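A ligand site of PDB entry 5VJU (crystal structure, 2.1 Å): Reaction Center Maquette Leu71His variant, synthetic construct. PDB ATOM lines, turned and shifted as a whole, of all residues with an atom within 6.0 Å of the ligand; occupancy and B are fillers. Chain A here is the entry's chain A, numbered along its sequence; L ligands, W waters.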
ATOM      1  N   ARG A   6      11.224 -29.188 -17.083  1.00  0.00           N
ATOM      2  CA  ARG A   6       9.857 -29.678 -17.244  1.00  0.00           C
ATOM      3  C   ARG A   6       9.512 -30.654 -16.132  1.00  0.00           C
ATOM      4  O   ARG A   6       8.483 -30.523 -15.529  1.00  0.00           O
ATOM      5  CB  ARG A   6       9.655 -30.307 -18.612  1.00  0.00           C
ATOM      6  CG  ARG A   6       8.353 -31.076 -18.756  1.00  0.00           C
ATOM      7  CD  ARG A   6       8.186 -31.612 -20.168  1.00  0.00           C
ATOM      8  NE  ARG A   6       6.863 -32.189 -20.303  1.00  0.00           N
ATOM      9  CZ  ARG A   6       6.351 -32.675 -21.418  1.00  0.00           C
ATOM     10  NH1 ARG A   6       7.047 -32.675 -22.544  1.00  0.00           N
ATOM     11  NH2 ARG A   6       5.121 -33.148 -21.408  1.00  0.00           N
ATOM     12  N   HIS A   9       9.118 -28.912 -12.621  1.00  0.00           N
ATOM     13  CA  HIS A   9       7.834 -28.265 -12.538  1.00  0.00           C
ATOM     14  C   HIS A   9       6.757 -29.264 -12.252  1.00  0.00           C
ATOM     15  O   HIS A   9       5.895 -29.041 -11.354  1.00  0.00           O
ATOM     16  CB  HIS A   9       7.566 -27.582 -13.891  1.00  0.00           C
ATOM     17  CG  HIS A   9       6.518 -26.535 -13.826  1.00  0.00           C
ATOM     18  ND1 HIS A   9       6.701 -25.330 -13.175  1.00  0.00           N
ATOM     19  CD2 HIS A   9       5.285 -26.508 -14.367  1.00  0.00           C
ATOM     20  CE1 HIS A   9       5.591 -24.626 -13.297  1.00  0.00           C
ATOM     21  NE2 HIS A   9       4.738 -25.299 -14.049  1.00  0.00           N
ATOM     22  N   GLN A  10       6.782 -30.346 -13.019  1.00  0.00           N
ATOM     23  CA  GLN A  10       5.834 -31.456 -12.821  1.00  0.00           C
ATOM     24  C   GLN A  10       5.870 -32.016 -11.343  1.00  0.00           C
ATOM     25  O   GLN A  10       4.842 -32.206 -10.695  1.00  0.00           O
ATOM     26  CB  GLN A  10       6.143 -32.531 -13.865  1.00  0.00           C
ATOM     27  CG  GLN A  10       4.985 -33.451 -14.197  1.00  0.00           C
ATOM     28  CD  GLN A  10       4.065 -32.839 -15.244  1.00  0.00           C
ATOM     29  OE1 GLN A  10       3.677 -31.678 -15.122  1.00  0.00           O
ATOM     30  NE2 GLN A  10       3.735 -33.592 -16.305  1.00  0.00           N
ATOM     31  N   LEU A  12       7.084 -30.500  -8.569  1.00  0.00           N
ATOM     32  CA  LEU A  12       6.627 -29.474  -7.621  1.00  0.00           C
ATOM     33  C   LEU A  12       5.113 -29.522  -7.519  1.00  0.00           C
ATOM     34  O   LEU A  12       4.568 -29.484  -6.443  1.00  0.00           O
ATOM     35  CB  LEU A  12       7.077 -28.064  -8.082  1.00  0.00           C
ATOM     36  CG  LEU A  12       8.594 -27.806  -7.998  1.00  0.00           C
ATOM     37  CD1 LEU A  12       9.016 -26.561  -8.795  1.00  0.00           C
ATOM     38  CD2 LEU A  12       9.105 -27.735  -6.577  1.00  0.00           C
ATOM     39  N   ALA A  13       4.456 -29.622  -8.664  1.00  0.00           N
ATOM     40  CA  ALA A  13       3.004 -29.678  -8.752  1.00  0.00           C
ATOM     41  C   ALA A  13       2.403 -30.941  -8.107  1.00  0.00           C
ATOM     42  O   ALA A  13       1.362 -30.856  -7.490  1.00  0.00           O
ATOM     43  CB  ALA A  13       2.601 -29.542 -10.183  1.00  0.00           C
ATOM     44  N   PHE A  16       2.834 -30.376  -4.446  1.00  0.00           N
ATOM     45  CA  PHE A  16       1.839 -29.361  -4.038  1.00  0.00           C
ATOM     46  C   PHE A  16       0.452 -30.029  -3.832  1.00  0.00           C
ATOM     47  O   PHE A  16      -0.197 -29.785  -2.830  1.00  0.00           O
ATOM     48  CB  PHE A  16       1.778 -28.254  -5.111  1.00  0.00           C
ATOM     49  CG  PHE A  16       0.822 -27.167  -4.795  1.00  0.00           C
ATOM     50  CD1 PHE A  16       1.009 -26.348  -3.721  1.00  0.00           C
ATOM     51  CD2 PHE A  16      -0.322 -26.998  -5.547  1.00  0.00           C
ATOM     52  CE1 PHE A  16       0.085 -25.346  -3.399  1.00  0.00           C
ATOM     53  CE2 PHE A  16      -1.234 -25.967  -5.264  1.00  0.00           C
ATOM     54  CZ  PHE A  16      -1.012 -25.130  -4.177  1.00  0.00           C
ATOM     55  N   LEU A  85      -5.872 -26.171  -8.782  1.00  0.00           N
ATOM     56  CA  LEU A  85      -4.814 -27.082  -9.041  1.00  0.00           C
ATOM     57  C   LEU A  85      -5.156 -28.102 -10.138  1.00  0.00           C
ATOM     58  O   LEU A  85      -4.315 -28.458 -10.960  1.00  0.00           O
ATOM     59  CB  LEU A  85      -4.432 -27.798  -7.743  1.00  0.00           C
ATOM     60  CG  LEU A  85      -3.231 -28.749  -7.755  1.00  0.00           C
ATOM     61  CD1 LEU A  85      -3.639 -30.162  -8.050  1.00  0.00           C
ATOM     62  CD2 LEU A  85      -2.141 -28.322  -8.726  1.00  0.00           C
ATOM     63  N   LEU A  88      -4.856 -26.252 -13.219  1.00  0.00           N
ATOM     64  CA  LEU A  88      -3.409 -26.065 -13.558  1.00  0.00           C
ATOM     65  C   LEU A  88      -2.840 -27.289 -14.266  1.00  0.00           C
ATOM     66  O   LEU A  88      -2.205 -27.178 -15.283  1.00  0.00           O
ATOM     67  CB  LEU A  88      -2.545 -25.671 -12.310  1.00  0.00           C
ATOM     68  CG  LEU A  88      -2.758 -24.171 -11.984  1.00  0.00           C
ATOM     69  CD1 LEU A  88      -2.555 -23.798 -10.531  1.00  0.00           C
ATOM     70  CD2 LEU A  88      -1.989 -23.268 -12.910  1.00  0.00           C
ATOM     71  N   GLN A  89      -3.124 -28.448 -13.723  1.00  0.00           N
ATOM     72  CA  GLN A  89      -2.682 -29.701 -14.290  1.00  0.00           C
ATOM     73  C   GLN A  89      -3.186 -29.863 -15.687  1.00  0.00           C
ATOM     74  O   GLN A  89      -2.422 -30.191 -16.538  1.00  0.00           O
ATOM     75  CB  GLN A  89      -3.206 -30.881 -13.464  1.00  0.00           C
ATOM     76  CG  GLN A  89      -2.579 -31.001 -12.069  1.00  0.00           C
ATOM     77  CD  GLN A  89      -3.286 -31.986 -11.129  1.00  0.00           C
ATOM     78  OE1 GLN A  89      -4.433 -32.427 -11.365  1.00  0.00           O
ATOM     79  NE2 GLN A  89      -2.598 -32.369 -10.074  1.00  0.00           N
ATOM     80  N   GLN A  90      -4.484 -29.658 -15.871  1.00  0.00           N
ATOM     81  CA  GLN A  90      -5.119 -29.790 -17.150  1.00  0.00           C
ATOM     82  C   GLN A  90      -4.623 -28.795 -18.203  1.00  0.00           C
ATOM     83  O   GLN A  90      -4.281 -29.190 -19.320  1.00  0.00           O
ATOM     84  CB  GLN A  90      -6.608 -29.620 -16.956  1.00  0.00           C
ATOM     85  CG  GLN A  90      -7.480 -29.756 -18.171  1.00  0.00           C
ATOM     86  CD  GLN A  90      -8.954 -29.623 -17.784  1.00  0.00           C
ATOM     87  OE1 GLN A  90      -9.303 -29.536 -16.603  1.00  0.00           O
ATOM     88  NE2 GLN A  90      -9.828 -29.591 -18.794  1.00  0.00           N
ATOM     89  N   THR A  91      -4.563 -27.511 -17.855  1.00  0.00           N
ATOM     90  CA  THR A  91      -4.054 -26.527 -18.789  1.00  0.00           C
ATOM     91  C   THR A  91      -2.617 -26.769 -19.060  1.00  0.00           C
ATOM     92  O   THR A  91      -2.177 -26.525 -20.158  1.00  0.00           O
ATOM     93  CB  THR A  91      -4.173 -25.051 -18.348  1.00  0.00           C
ATOM     94  OG1 THR A  91      -3.658 -24.858 -17.028  1.00  0.00           O
ATOM     95  CG2 THR A  91      -5.590 -24.514 -18.463  1.00  0.00           C
ATOM     96  N   GLY A  92      -1.875 -27.214 -18.032  1.00  0.00           N
ATOM     97  CA  GLY A  92      -0.426 -27.522 -18.176  1.00  0.00           C
ATOM     98  C   GLY A  92      -0.110 -28.571 -19.213  1.00  0.00           C
ATOM     99  O   GLY A  92       0.787 -28.376 -20.039  1.00  0.00           O
ATOM    100  N   GLN A  93      -0.780 -29.720 -19.102  1.00  0.00           N
ATOM    101  CA  GLN A  93      -0.667 -30.828 -20.041  1.00  0.00           C
ATOM    102  C   GLN A  93      -1.054 -30.412 -21.433  1.00  0.00           C
ATOM    103  O   GLN A  93      -0.428 -30.814 -22.410  1.00  0.00           O
ATOM    104  CB  GLN A  93      -1.630 -31.957 -19.659  1.00  0.00           C
ATOM    105  CG  GLN A  93      -1.184 -32.737 -18.417  1.00  0.00           C
ATOM    106  CD  GLN A  93      -2.336 -33.396 -17.626  1.00  0.00           C
ATOM    107  OE1 GLN A  93      -3.530 -33.272 -17.962  1.00  0.00           O
ATOM    108  NE2 GLN A  93      -1.981 -34.084 -16.591  1.00  0.00           N
ATOM    109  N   LEU A  95      -0.814 -27.347 -22.674  1.00  0.00           N
ATOM    110  CA  LEU A  95       0.317 -26.522 -23.138  1.00  0.00           C
ATOM    111  C   LEU A  95       1.485 -27.291 -23.692  1.00  0.00           C
ATOM    112  O   LEU A  95       2.062 -26.920 -24.722  1.00  0.00           O
ATOM    113  CB  LEU A  95       0.808 -25.552 -22.037  1.00  0.00           C
ATOM    114  CG  LEU A  95      -0.109 -24.331 -21.784  1.00  0.00           C
ATOM    115  CD1 LEU A  95       0.236 -23.702 -20.424  1.00  0.00           C
ATOM    116  CD2 LEU A  95      -0.039 -23.283 -22.914  1.00  0.00           C
ATOM    117  N   TRP A  96       1.866 -28.372 -23.016  1.00  0.00           N
ATOM    118  CA  TRP A  96       2.921 -29.233 -23.532  1.00  0.00           C
ATOM    119  C   TRP A  96       2.527 -29.970 -24.797  1.00  0.00           C
ATOM    120  O   TRP A  96       3.300 -30.045 -25.762  1.00  0.00           O
ATOM    121  CB  TRP A  96       3.380 -30.252 -22.491  1.00  0.00           C
ATOM    122  CG  TRP A  96       4.397 -29.666 -21.541  1.00  0.00           C
ATOM    123  CD1 TRP A  96       4.280 -29.583 -20.208  1.00  0.00           C
ATOM    124  CD2 TRP A  96       5.664 -29.090 -21.887  1.00  0.00           C
ATOM    125  NE1 TRP A  96       5.388 -28.975 -19.659  1.00  0.00           N
ATOM    126  CE2 TRP A  96       6.266 -28.690 -20.677  1.00  0.00           C
ATOM    127  CE3 TRP A  96       6.350 -28.892 -23.095  1.00  0.00           C
ATOM    128  CZ2 TRP A  96       7.530 -28.071 -20.643  1.00  0.00           C
ATOM    129  CZ3 TRP A  96       7.634 -28.287 -23.059  1.00  0.00           C
ATOM    130  CH2 TRP A  96       8.200 -27.888 -21.838  1.00  0.00           C
ATOM    131  N   LEU A 106      -4.720 -20.082 -23.781  1.00  0.00           N
ATOM    132  CA  LEU A 106      -4.237 -21.206 -22.950  1.00  0.00           C
ATOM    133  C   LEU A 106      -3.117 -20.796 -21.986  1.00  0.00           C
ATOM    134  O   LEU A 106      -3.147 -21.136 -20.775  1.00  0.00           O
ATOM    135  CB  LEU A 106      -3.753 -22.365 -23.850  1.00  0.00           C
ATOM    136  CG  LEU A 106      -3.468 -23.681 -23.121  1.00  0.00           C
ATOM    137  CD1 LEU A 106      -4.727 -24.203 -22.460  1.00  0.00           C
ATOM    138  CD2 LEU A 106      -2.917 -24.712 -24.064  1.00  0.00           C
ATOM    139  N   ARG A 107      -2.111 -20.076 -22.496  1.00  0.00           N
ATOM    140  CA  ARG A 107      -0.965 -19.641 -21.660  1.00  0.00           C
ATOM    141  C   ARG A 107      -1.441 -18.639 -20.592  1.00  0.00           C
ATOM    142  O   ARG A 107      -0.957 -18.646 -19.464  1.00  0.00           O
ATOM    143  CB  ARG A 107       0.184 -19.077 -22.520  1.00  0.00           C
ATOM    144  CG  ARG A 107       1.330 -18.376 -21.779  1.00  0.00           C
ATOM    145  CD  ARG A 107       2.538 -18.100 -22.699  1.00  0.00           C
ATOM    146  NE  ARG A 107       2.126 -17.602 -24.030  1.00  0.00           N
ATOM    147  CZ  ARG A 107       1.709 -16.356 -24.304  1.00  0.00           C
ATOM    148  NH1 ARG A 107       1.675 -15.404 -23.367  1.00  0.00           N
ATOM    149  NH2 ARG A 107       1.346 -16.051 -25.550  1.00  0.00           N
ATOM    150  N   GLN A 108      -2.414 -17.811 -20.940  1.00  0.00           N
ATOM    151  CA  GLN A 108      -2.966 -16.800 -20.035  1.00  0.00           C
ATOM    152  C   GLN A 108      -3.779 -17.439 -18.942  1.00  0.00           C
ATOM    153  O   GLN A 108      -3.739 -16.989 -17.772  1.00  0.00           O
ATOM    154  CB  GLN A 108      -3.820 -15.773 -20.828  1.00  0.00           C
ATOM    155  CG  GLN A 108      -2.979 -14.913 -21.779  1.00  0.00           C
ATOM    156  CD  GLN A 108      -3.737 -14.341 -22.995  1.00  0.00           C
ATOM    157  OE1 GLN A 108      -4.967 -14.354 -23.045  1.00  0.00           O
ATOM    158  NE2 GLN A 108      -2.990 -13.834 -23.971  1.00  0.00           N
ATOM    159  N   HIS A 110      -3.306 -20.446 -17.598  1.00  0.00           N
ATOM    160  CA  HIS A 110      -2.423 -21.130 -16.704  1.00  0.00           C
ATOM    161  C   HIS A 110      -1.763 -20.083 -15.761  1.00  0.00           C
ATOM    162  O   HIS A 110      -1.706 -20.275 -14.541  1.00  0.00           O
ATOM    163  CB  HIS A 110      -1.359 -21.867 -17.513  1.00  0.00           C
ATOM    164  CG  HIS A 110      -0.601 -22.894 -16.739  1.00  0.00           C
ATOM    165  ND1 HIS A 110      -1.092 -24.158 -16.483  1.00  0.00           N
ATOM    166  CD2 HIS A 110       0.630 -22.842 -16.183  1.00  0.00           C
ATOM    167  CE1 HIS A 110      -0.193 -24.839 -15.799  1.00  0.00           C
ATOM    168  NE2 HIS A 110       0.851 -24.061 -15.592  1.00  0.00           N
ATOM    169  N   GLN A 111      -1.302 -18.993 -16.342  1.00  0.00           N
ATOM    170  CA  GLN A 111      -0.753 -17.872 -15.547  1.00  0.00           C
ATOM    171  C   GLN A 111      -1.797 -17.309 -14.574  1.00  0.00           C
ATOM    172  O   GLN A 111      -1.499 -17.143 -13.421  1.00  0.00           O
ATOM    173  CB  GLN A 111      -0.202 -16.755 -16.455  1.00  0.00           C
ATOM    174  CG  GLN A 111       0.616 -15.694 -15.681  1.00  0.00           C
ATOM    175  CD  GLN A 111      -0.235 -14.720 -14.843  1.00  0.00           C
ATOM    176  OE1 GLN A 111      -1.356 -14.385 -15.201  1.00  0.00           O
ATOM    177  NE2 GLN A 111       0.328 -14.248 -13.731  1.00  0.00           N
ATOM    178  N   ALA A 114      -2.442 -19.574 -11.686  1.00  0.00           N
ATOM    179  CA  ALA A 114      -1.316 -19.481 -10.724  1.00  0.00           C
ATOM    180  C   ALA A 114      -1.462 -18.269  -9.802  1.00  0.00           C
ATOM    181  O   ALA A 114      -1.346 -18.355  -8.559  1.00  0.00           O
ATOM    182  CB  ALA A 114       0.008 -19.425 -11.463  1.00  0.00           C
ATOM    183  N   ILE A 117      -4.496 -18.931  -7.302  1.00  0.00           N
ATOM    184  CA  ILE A 117      -4.224 -19.932  -6.282  1.00  0.00           C
ATOM    185  C   ILE A 117      -3.290 -19.334  -5.231  1.00  0.00           C
ATOM    186  O   ILE A 117      -3.478 -19.586  -4.078  1.00  0.00           O
ATOM    187  CB  ILE A 117      -3.705 -21.295  -6.887  1.00  0.00           C
ATOM    188  CG1 ILE A 117      -3.983 -22.468  -5.935  1.00  0.00           C
ATOM    189  CG2 ILE A 117      -2.241 -21.263  -7.259  1.00  0.00           C
ATOM    190  CD1 ILE A 117      -3.699 -23.840  -6.548  1.00  0.00           C
ATOM    191  N   VAL A 182       4.403 -22.795  -4.601  1.00  0.00           N
ATOM    192  CA  VAL A 182       3.842 -21.910  -5.660  1.00  0.00           C
ATOM    193  C   VAL A 182       4.877 -20.936  -6.222  1.00  0.00           C
ATOM    194  O   VAL A 182       4.986 -20.792  -7.462  1.00  0.00           O
ATOM    195  CB  VAL A 182       2.565 -21.181  -5.187  1.00  0.00           C
ATOM    196  CG1 VAL A 182       2.159 -20.058  -6.159  1.00  0.00           C
ATOM    197  CG2 VAL A 182       1.423 -22.175  -5.058  1.00  0.00           C
ATOM    198  N   LEU A 185       7.061 -22.969  -8.444  1.00  0.00           N
ATOM    199  CA  LEU A 185       6.379 -23.338  -9.660  1.00  0.00           C
ATOM    200  C   LEU A 185       6.363 -22.143 -10.622  1.00  0.00           C
ATOM    201  O   LEU A 185       6.636 -22.293 -11.799  1.00  0.00           O
ATOM    202  CB  LEU A 185       4.974 -23.814  -9.357  1.00  0.00           C
ATOM    203  CG  LEU A 185       4.855 -25.270  -8.861  1.00  0.00           C
ATOM    204  CD1 LEU A 185       3.613 -25.441  -7.996  1.00  0.00           C
ATOM    205  CD2 LEU A 185       4.801 -26.226 -10.045  1.00  0.00           C
ATOM    206  N   GLN A 186       6.146 -20.935 -10.120  1.00  0.00           N
ATOM    207  CA  GLN A 186       6.283 -19.747 -10.949  1.00  0.00           C
ATOM    208  C   GLN A 186       7.705 -19.575 -11.503  1.00  0.00           C
ATOM    209  O   GLN A 186       7.893 -19.184 -12.672  1.00  0.00           O
ATOM    210  CB  GLN A 186       5.917 -18.494 -10.132  1.00  0.00           C
ATOM    211  CG  GLN A 186       6.208 -17.206 -10.896  1.00  0.00           C
ATOM    212  CD  GLN A 186       5.511 -16.017 -10.305  1.00  0.00           C
ATOM    213  OE1 GLN A 186       5.570 -15.792  -9.097  1.00  0.00           O
ATOM    214  NE2 GLN A 186       4.864 -15.241 -11.162  1.00  0.00           N
ATOM    215  N   GLN A 187       8.692 -19.786 -10.655  1.00  0.00           N
ATOM    216  CA  GLN A 187      10.091 -19.548 -11.025  1.00  0.00           C
ATOM    217  C   GLN A 187      10.515 -20.563 -12.106  1.00  0.00           C
ATOM    218  O   GLN A 187      11.147 -20.194 -13.098  1.00  0.00           O
ATOM    219  CB  GLN A 187      10.960 -19.611  -9.763  1.00  0.00           C
ATOM    220  CG  GLN A 187      12.452 -19.434  -9.935  1.00  0.00           C
ATOM    221  CD  GLN A 187      13.212 -20.018  -8.730  1.00  0.00           C
ATOM    222  OE1 GLN A 187      13.957 -20.976  -8.881  1.00  0.00           O
ATOM    223  NE2 GLN A 187      12.967 -19.470  -7.548  1.00  0.00           N
ATOM    224  N   THR A 188      10.180 -21.842 -11.901  1.00  0.00           N
ATOM    225  CA  THR A 188      10.471 -22.874 -12.918  1.00  0.00           C
ATOM    226  C   THR A 188       9.591 -22.694 -14.182  1.00  0.00           C
ATOM    227  O   THR A 188      10.056 -22.868 -15.322  1.00  0.00           O
ATOM    228  CB  THR A 188      10.273 -24.314 -12.403  1.00  0.00           C
ATOM    229  OG1 THR A 188       8.984 -24.465 -11.803  1.00  0.00           O
ATOM    230  CG2 THR A 188      11.325 -24.674 -11.359  1.00  0.00           C
ATOM    231  N   GLY A 189       8.324 -22.414 -13.947  1.00  0.00           N
ATOM    232  CA  GLY A 189       7.304 -22.267 -15.017  1.00  0.00           C
ATOM    233  C   GLY A 189       7.689 -21.219 -16.072  1.00  0.00           C
ATOM    234  O   GLY A 189       7.646 -21.498 -17.259  1.00  0.00           O
ATOM    235  N   GLN A 190       8.210 -20.083 -15.602  1.00  0.00           N
ATOM    236  CA  GLN A 190       8.649 -18.969 -16.468  1.00  0.00           C
ATOM    237  C   GLN A 190       9.826 -19.335 -17.347  1.00  0.00           C
ATOM    238  O   GLN A 190       9.951 -18.809 -18.443  1.00  0.00           O
ATOM    239  CB  GLN A 190       8.973 -17.729 -15.629  1.00  0.00           C
ATOM    240  CG  GLN A 190       7.701 -17.081 -15.082  1.00  0.00           C
ATOM    241  CD  GLN A 190       7.923 -15.882 -14.146  1.00  0.00           C
ATOM    242  OE1 GLN A 190       7.080 -15.009 -14.093  1.00  0.00           O
ATOM    243  NE2 GLN A 190       9.013 -15.873 -13.386  1.00  0.00           N
ATOM    244  N   LEU A 192      10.291 -22.442 -18.579  1.00  0.00           N
ATOM    245  CA  LEU A 192      10.098 -23.726 -19.266  1.00  0.00           C
ATOM    246  C   LEU A 192      10.227 -23.647 -20.778  1.00  0.00           C
ATOM    247  O   LEU A 192      10.703 -24.602 -21.402  1.00  0.00           O
ATOM    248  CB  LEU A 192       8.759 -24.393 -18.902  1.00  0.00           C
ATOM    249  CG  LEU A 192       8.523 -25.043 -17.524  1.00  0.00           C
ATOM    250  CD1 LEU A 192       7.236 -25.909 -17.539  1.00  0.00           C
ATOM    251  CD2 LEU A 192       9.712 -25.850 -16.985  1.00  0.00           C
ATOM    252  N   TRP A 193       9.743 -22.564 -21.354  1.00  0.00           N
ATOM    253  CA  TRP A 193       9.747 -22.355 -22.799  1.00  0.00           C
ATOM    254  C   TRP A 193      10.737 -21.261 -23.189  1.00  0.00           C
ATOM    255  O   TRP A 193      10.587 -20.674 -24.257  1.00  0.00           O
ATOM    256  CB  TRP A 193       8.338 -21.986 -23.274  1.00  0.00           C
ATOM    257  CG  TRP A 193       7.351 -23.142 -23.302  1.00  0.00           C
ATOM    258  CD1 TRP A 193       7.558 -24.437 -22.872  1.00  0.00           C
ATOM    259  CD2 TRP A 193       5.999 -23.101 -23.767  1.00  0.00           C
ATOM    260  NE1 TRP A 193       6.421 -25.207 -23.071  1.00  0.00           N
ATOM    261  CE2 TRP A 193       5.449 -24.413 -23.616  1.00  0.00           C
ATOM    262  CE3 TRP A 193       5.199 -22.108 -24.327  1.00  0.00           C
ATOM    263  CZ2 TRP A 193       4.157 -24.726 -23.998  1.00  0.00           C
ATOM    264  CZ3 TRP A 193       3.879 -22.436 -24.679  1.00  0.00           C
ATOM    265  CH2 TRP A 193       3.387 -23.735 -24.524  1.00  0.00           C
HETATM  266  C1  LIG L   1       4.346 -22.374 -16.751  1.00  0.00           C
HETATM  267  C2  LIG L   1       2.391 -22.259 -12.388  1.00  0.00           C
HETATM  268  C3  LIG L   1       1.478 -26.985 -12.724  1.00  0.00           C
HETATM  269  C4  LIG L   1       2.770 -26.899 -17.349  1.00  0.00           C
HETATM  270  C5  LIG L   1       3.923 -21.935 -15.541  1.00  0.00           C
HETATM  271  C6  LIG L   1       4.039 -20.596 -15.053  1.00  0.00           C
HETATM  272  C7  LIG L   1       3.455 -20.565 -13.845  1.00  0.00           C
HETATM  273  C8  LIG L   1       3.016 -21.889 -13.556  1.00  0.00           C
HETATM  274  C9  LIG L   1       3.318 -19.337 -12.965  1.00  0.00           C
HETATM  275  C10 LIG L   1       4.612 -19.382 -15.769  1.00  0.00           C
HETATM  276  C11 LIG L   1       3.410 -18.751 -16.523  1.00  0.00           C
HETATM  277  C12 LIG L   1       3.855 -17.668 -17.484  1.00  0.00           C
HETATM  278  O1  LIG L   1       4.591 -17.948 -18.463  1.00  0.00           O
HETATM  279  O2  LIG L   1       3.469 -16.510 -17.288  1.00  0.00           O
HETATM  280  C13 LIG L   1       1.964 -23.562 -12.077  1.00  0.00           C
HETATM  281  C14 LIG L   1       1.427 -23.934 -10.785  1.00  0.00           C
HETATM  282  C15 LIG L   1       1.180 -25.265 -10.863  1.00  0.00           C
HETATM  283  C16 LIG L   1       1.604 -25.695 -12.230  1.00  0.00           C
HETATM  284  C17 LIG L   1       1.133 -23.028  -9.593  1.00  0.00           C
HETATM  285  C18 LIG L   1       0.640 -26.194  -9.875  1.00  0.00           C
HETATM  286  C19 LIG L   1       0.350 -25.913  -8.629  1.00  0.00           C
HETATM  287  C20 LIG L   1       1.715 -27.388 -14.026  1.00  0.00           C
HETATM  288  C21 LIG L   1       1.505 -28.680 -14.480  1.00  0.00           C
HETATM  289  C22 LIG L   1       1.882 -28.688 -15.797  1.00  0.00           C
HETATM  290  C23 LIG L   1       2.319 -27.359 -16.160  1.00  0.00           C
HETATM  291  C24 LIG L   1       1.001 -29.855 -13.665  1.00  0.00           C
HETATM  292  C25 LIG L   1       1.816 -29.961 -16.516  1.00  0.00           C
HETATM  293  C26 LIG L   1       2.522 -30.212 -17.551  1.00  0.00           C
HETATM  294  C27 LIG L   1       3.298 -25.644 -17.518  1.00  0.00           C
HETATM  295  C28 LIG L   1       3.900 -25.254 -18.799  1.00  0.00           C
HETATM  296  C29 LIG L   1       4.367 -24.009 -18.619  1.00  0.00           C
HETATM  297  C30 LIG L   1       4.041 -23.637 -17.247  1.00  0.00           C
HETATM  298  C31 LIG L   1       4.029 -26.020 -20.100  1.00  0.00           C
HETATM  299  C32 LIG L   1       5.102 -23.171 -19.671  1.00  0.00           C
HETATM  300  C33 LIG L   1       4.208 -22.357 -20.650  1.00  0.00           C
HETATM  301  C34 LIG L   1       3.541 -21.145 -20.061  1.00  0.00           C
HETATM  302  O3  LIG L   1       2.286 -21.110 -20.004  1.00  0.00           O
HETATM  303  O4  LIG L   1       4.232 -20.201 -19.617  1.00  0.00           O
HETATM  304  N1  LIG L   1       3.308 -22.708 -14.610  1.00  0.00           N
HETATM  305  N2  LIG L   1       2.062 -24.633 -12.877  1.00  0.00           N
HETATM  306  N3  LIG L   1       2.237 -26.637 -15.037  1.00  0.00           N
HETATM  307  N4  LIG L   1       3.420 -24.658 -16.615  1.00  0.00           N
HETATM  308 FE1  LIG L   1       2.774 -24.654 -14.840  1.00  0.00          FE
HETATM  309  O   HOH W   1       4.117 -15.516 -14.160  1.00  0.00           O
HETATM  310  O   HOH W   2       3.114 -20.305  -9.533  1.00  0.00           O
HETATM  311  O   HOH W   3       2.451 -32.893 -19.298  1.00  0.00           O
HETATM  312  O   HOH W   4       5.821 -29.695 -16.743  1.00  0.00           O
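A ring nitrogen (NE2) of His 110 is bound to an iron atom (FE1) of the ligand, 2.1 Å away.
An iron atom (FE1) of the ligand is bound by a ring nitrogen (NE2) of His 9 (2.2 Å).
ND1 of His 110 lies close to O of Leu 88 (3.4 Å).
A ring nitrogen (ND1) of His 110 is in hydrogen-bond range of the side-chain hydroxyl of Thr 91.
A ring nitrogen (ND1) of His 9 lies close to the backbone carbonyl oxygen of Leu 185 (3.3 Å).
ND1 of His 9 is in hydrogen-bond range of N of Gly 189, 3.4 Å away.
A ring nitrogen (ND1) of His 9 lies within hydrogen-bond range of the side-chain hydroxyl (OG1) of Thr 188.
O of Leu 185 sits at hydrogen-bond distance from OG1 of Thr 188 (3.2 Å).
The backbone carbonyl oxygen (O) of Leu 88 is in hydrogen-bond range of the side-chain hydroxyl (OG1) of Thr 91, at 3.2 Å.
Gln 10 touches the ligand.
Ala 13 touches the ligand (CB to C3, 3.8 Å).
CD2 of Phe 16 touches C19 of the ligand, at 3.3 Å.
Leu 85 touches the ligand (CD2 to C19, 3.5 Å).
Leu 88 touches the ligand.
Gln 89 touches the ligand.
Gly 92 touches the ligand (CA to C4, 3.4 Å).
N of Gln 93 touches C25 of the ligand (3.7 Å).
Leu 95 touches the ligand (CD1 to O3, 3.3 Å).
Trp 96 touches the ligand.
CG of Arg 107 touches O3 of the ligand (3.4 Å).
Gln 111 touches the ligand (CG to O2, 3.4 Å).
CB of Ala 114 touches C9 of the ligand, at 3.6 Å.
CD1 of Leu 185 touches C19 of the ligand (3.4 Å).
Gln 186 touches the ligand.
Gly 189 touches the ligand.
N of Gln 190 touches C10 of the ligand (3.7 Å).
Leu 192 touches the ligand (CD1 to C29, 3.6 Å).
Trp 193 touches the ligand.
Hydrophobic or aromatic side chains that line the ligand: His 9, Ala 13, Phe 16, Leu 85, Leu 88, Leu 95, Trp 96, His 110, Ala 114, Leu 185, Leu 192 and Trp 193.
Within 4 Å of the ligand: His 9, Gln 10, Ala 13, Phe 16, Leu 85, Leu 88, Gln 89, Gly 92, Gln 93, Leu 95, Trp 96, Arg 107, His 110, Gln 111, Ala 114, Leu 185, Gln 186, Gly 189, Gln 190, Leu 192 and Trp 193.
Water W3 lies within hydrogen-bond range of the side-chain amide nitrogen (NE2) of Gln 10 and the guanidinium group (NH2) of Arg 6.
Water W1 lies within hydrogen-bond range of OE1 of Gln 190 (3.0 Å), NE2 of Gln 186 (3.1 Å) and O2 of the ligand (3.3 Å).
Water W4 lies within hydrogen-bond range of the indole nitrogen of Trp 96 (3.0 Å), the backbone carbonyl oxygen of Arg 6 (3.0 Å) and the side-chain amide oxygen of Gln 10 (3.3 Å).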
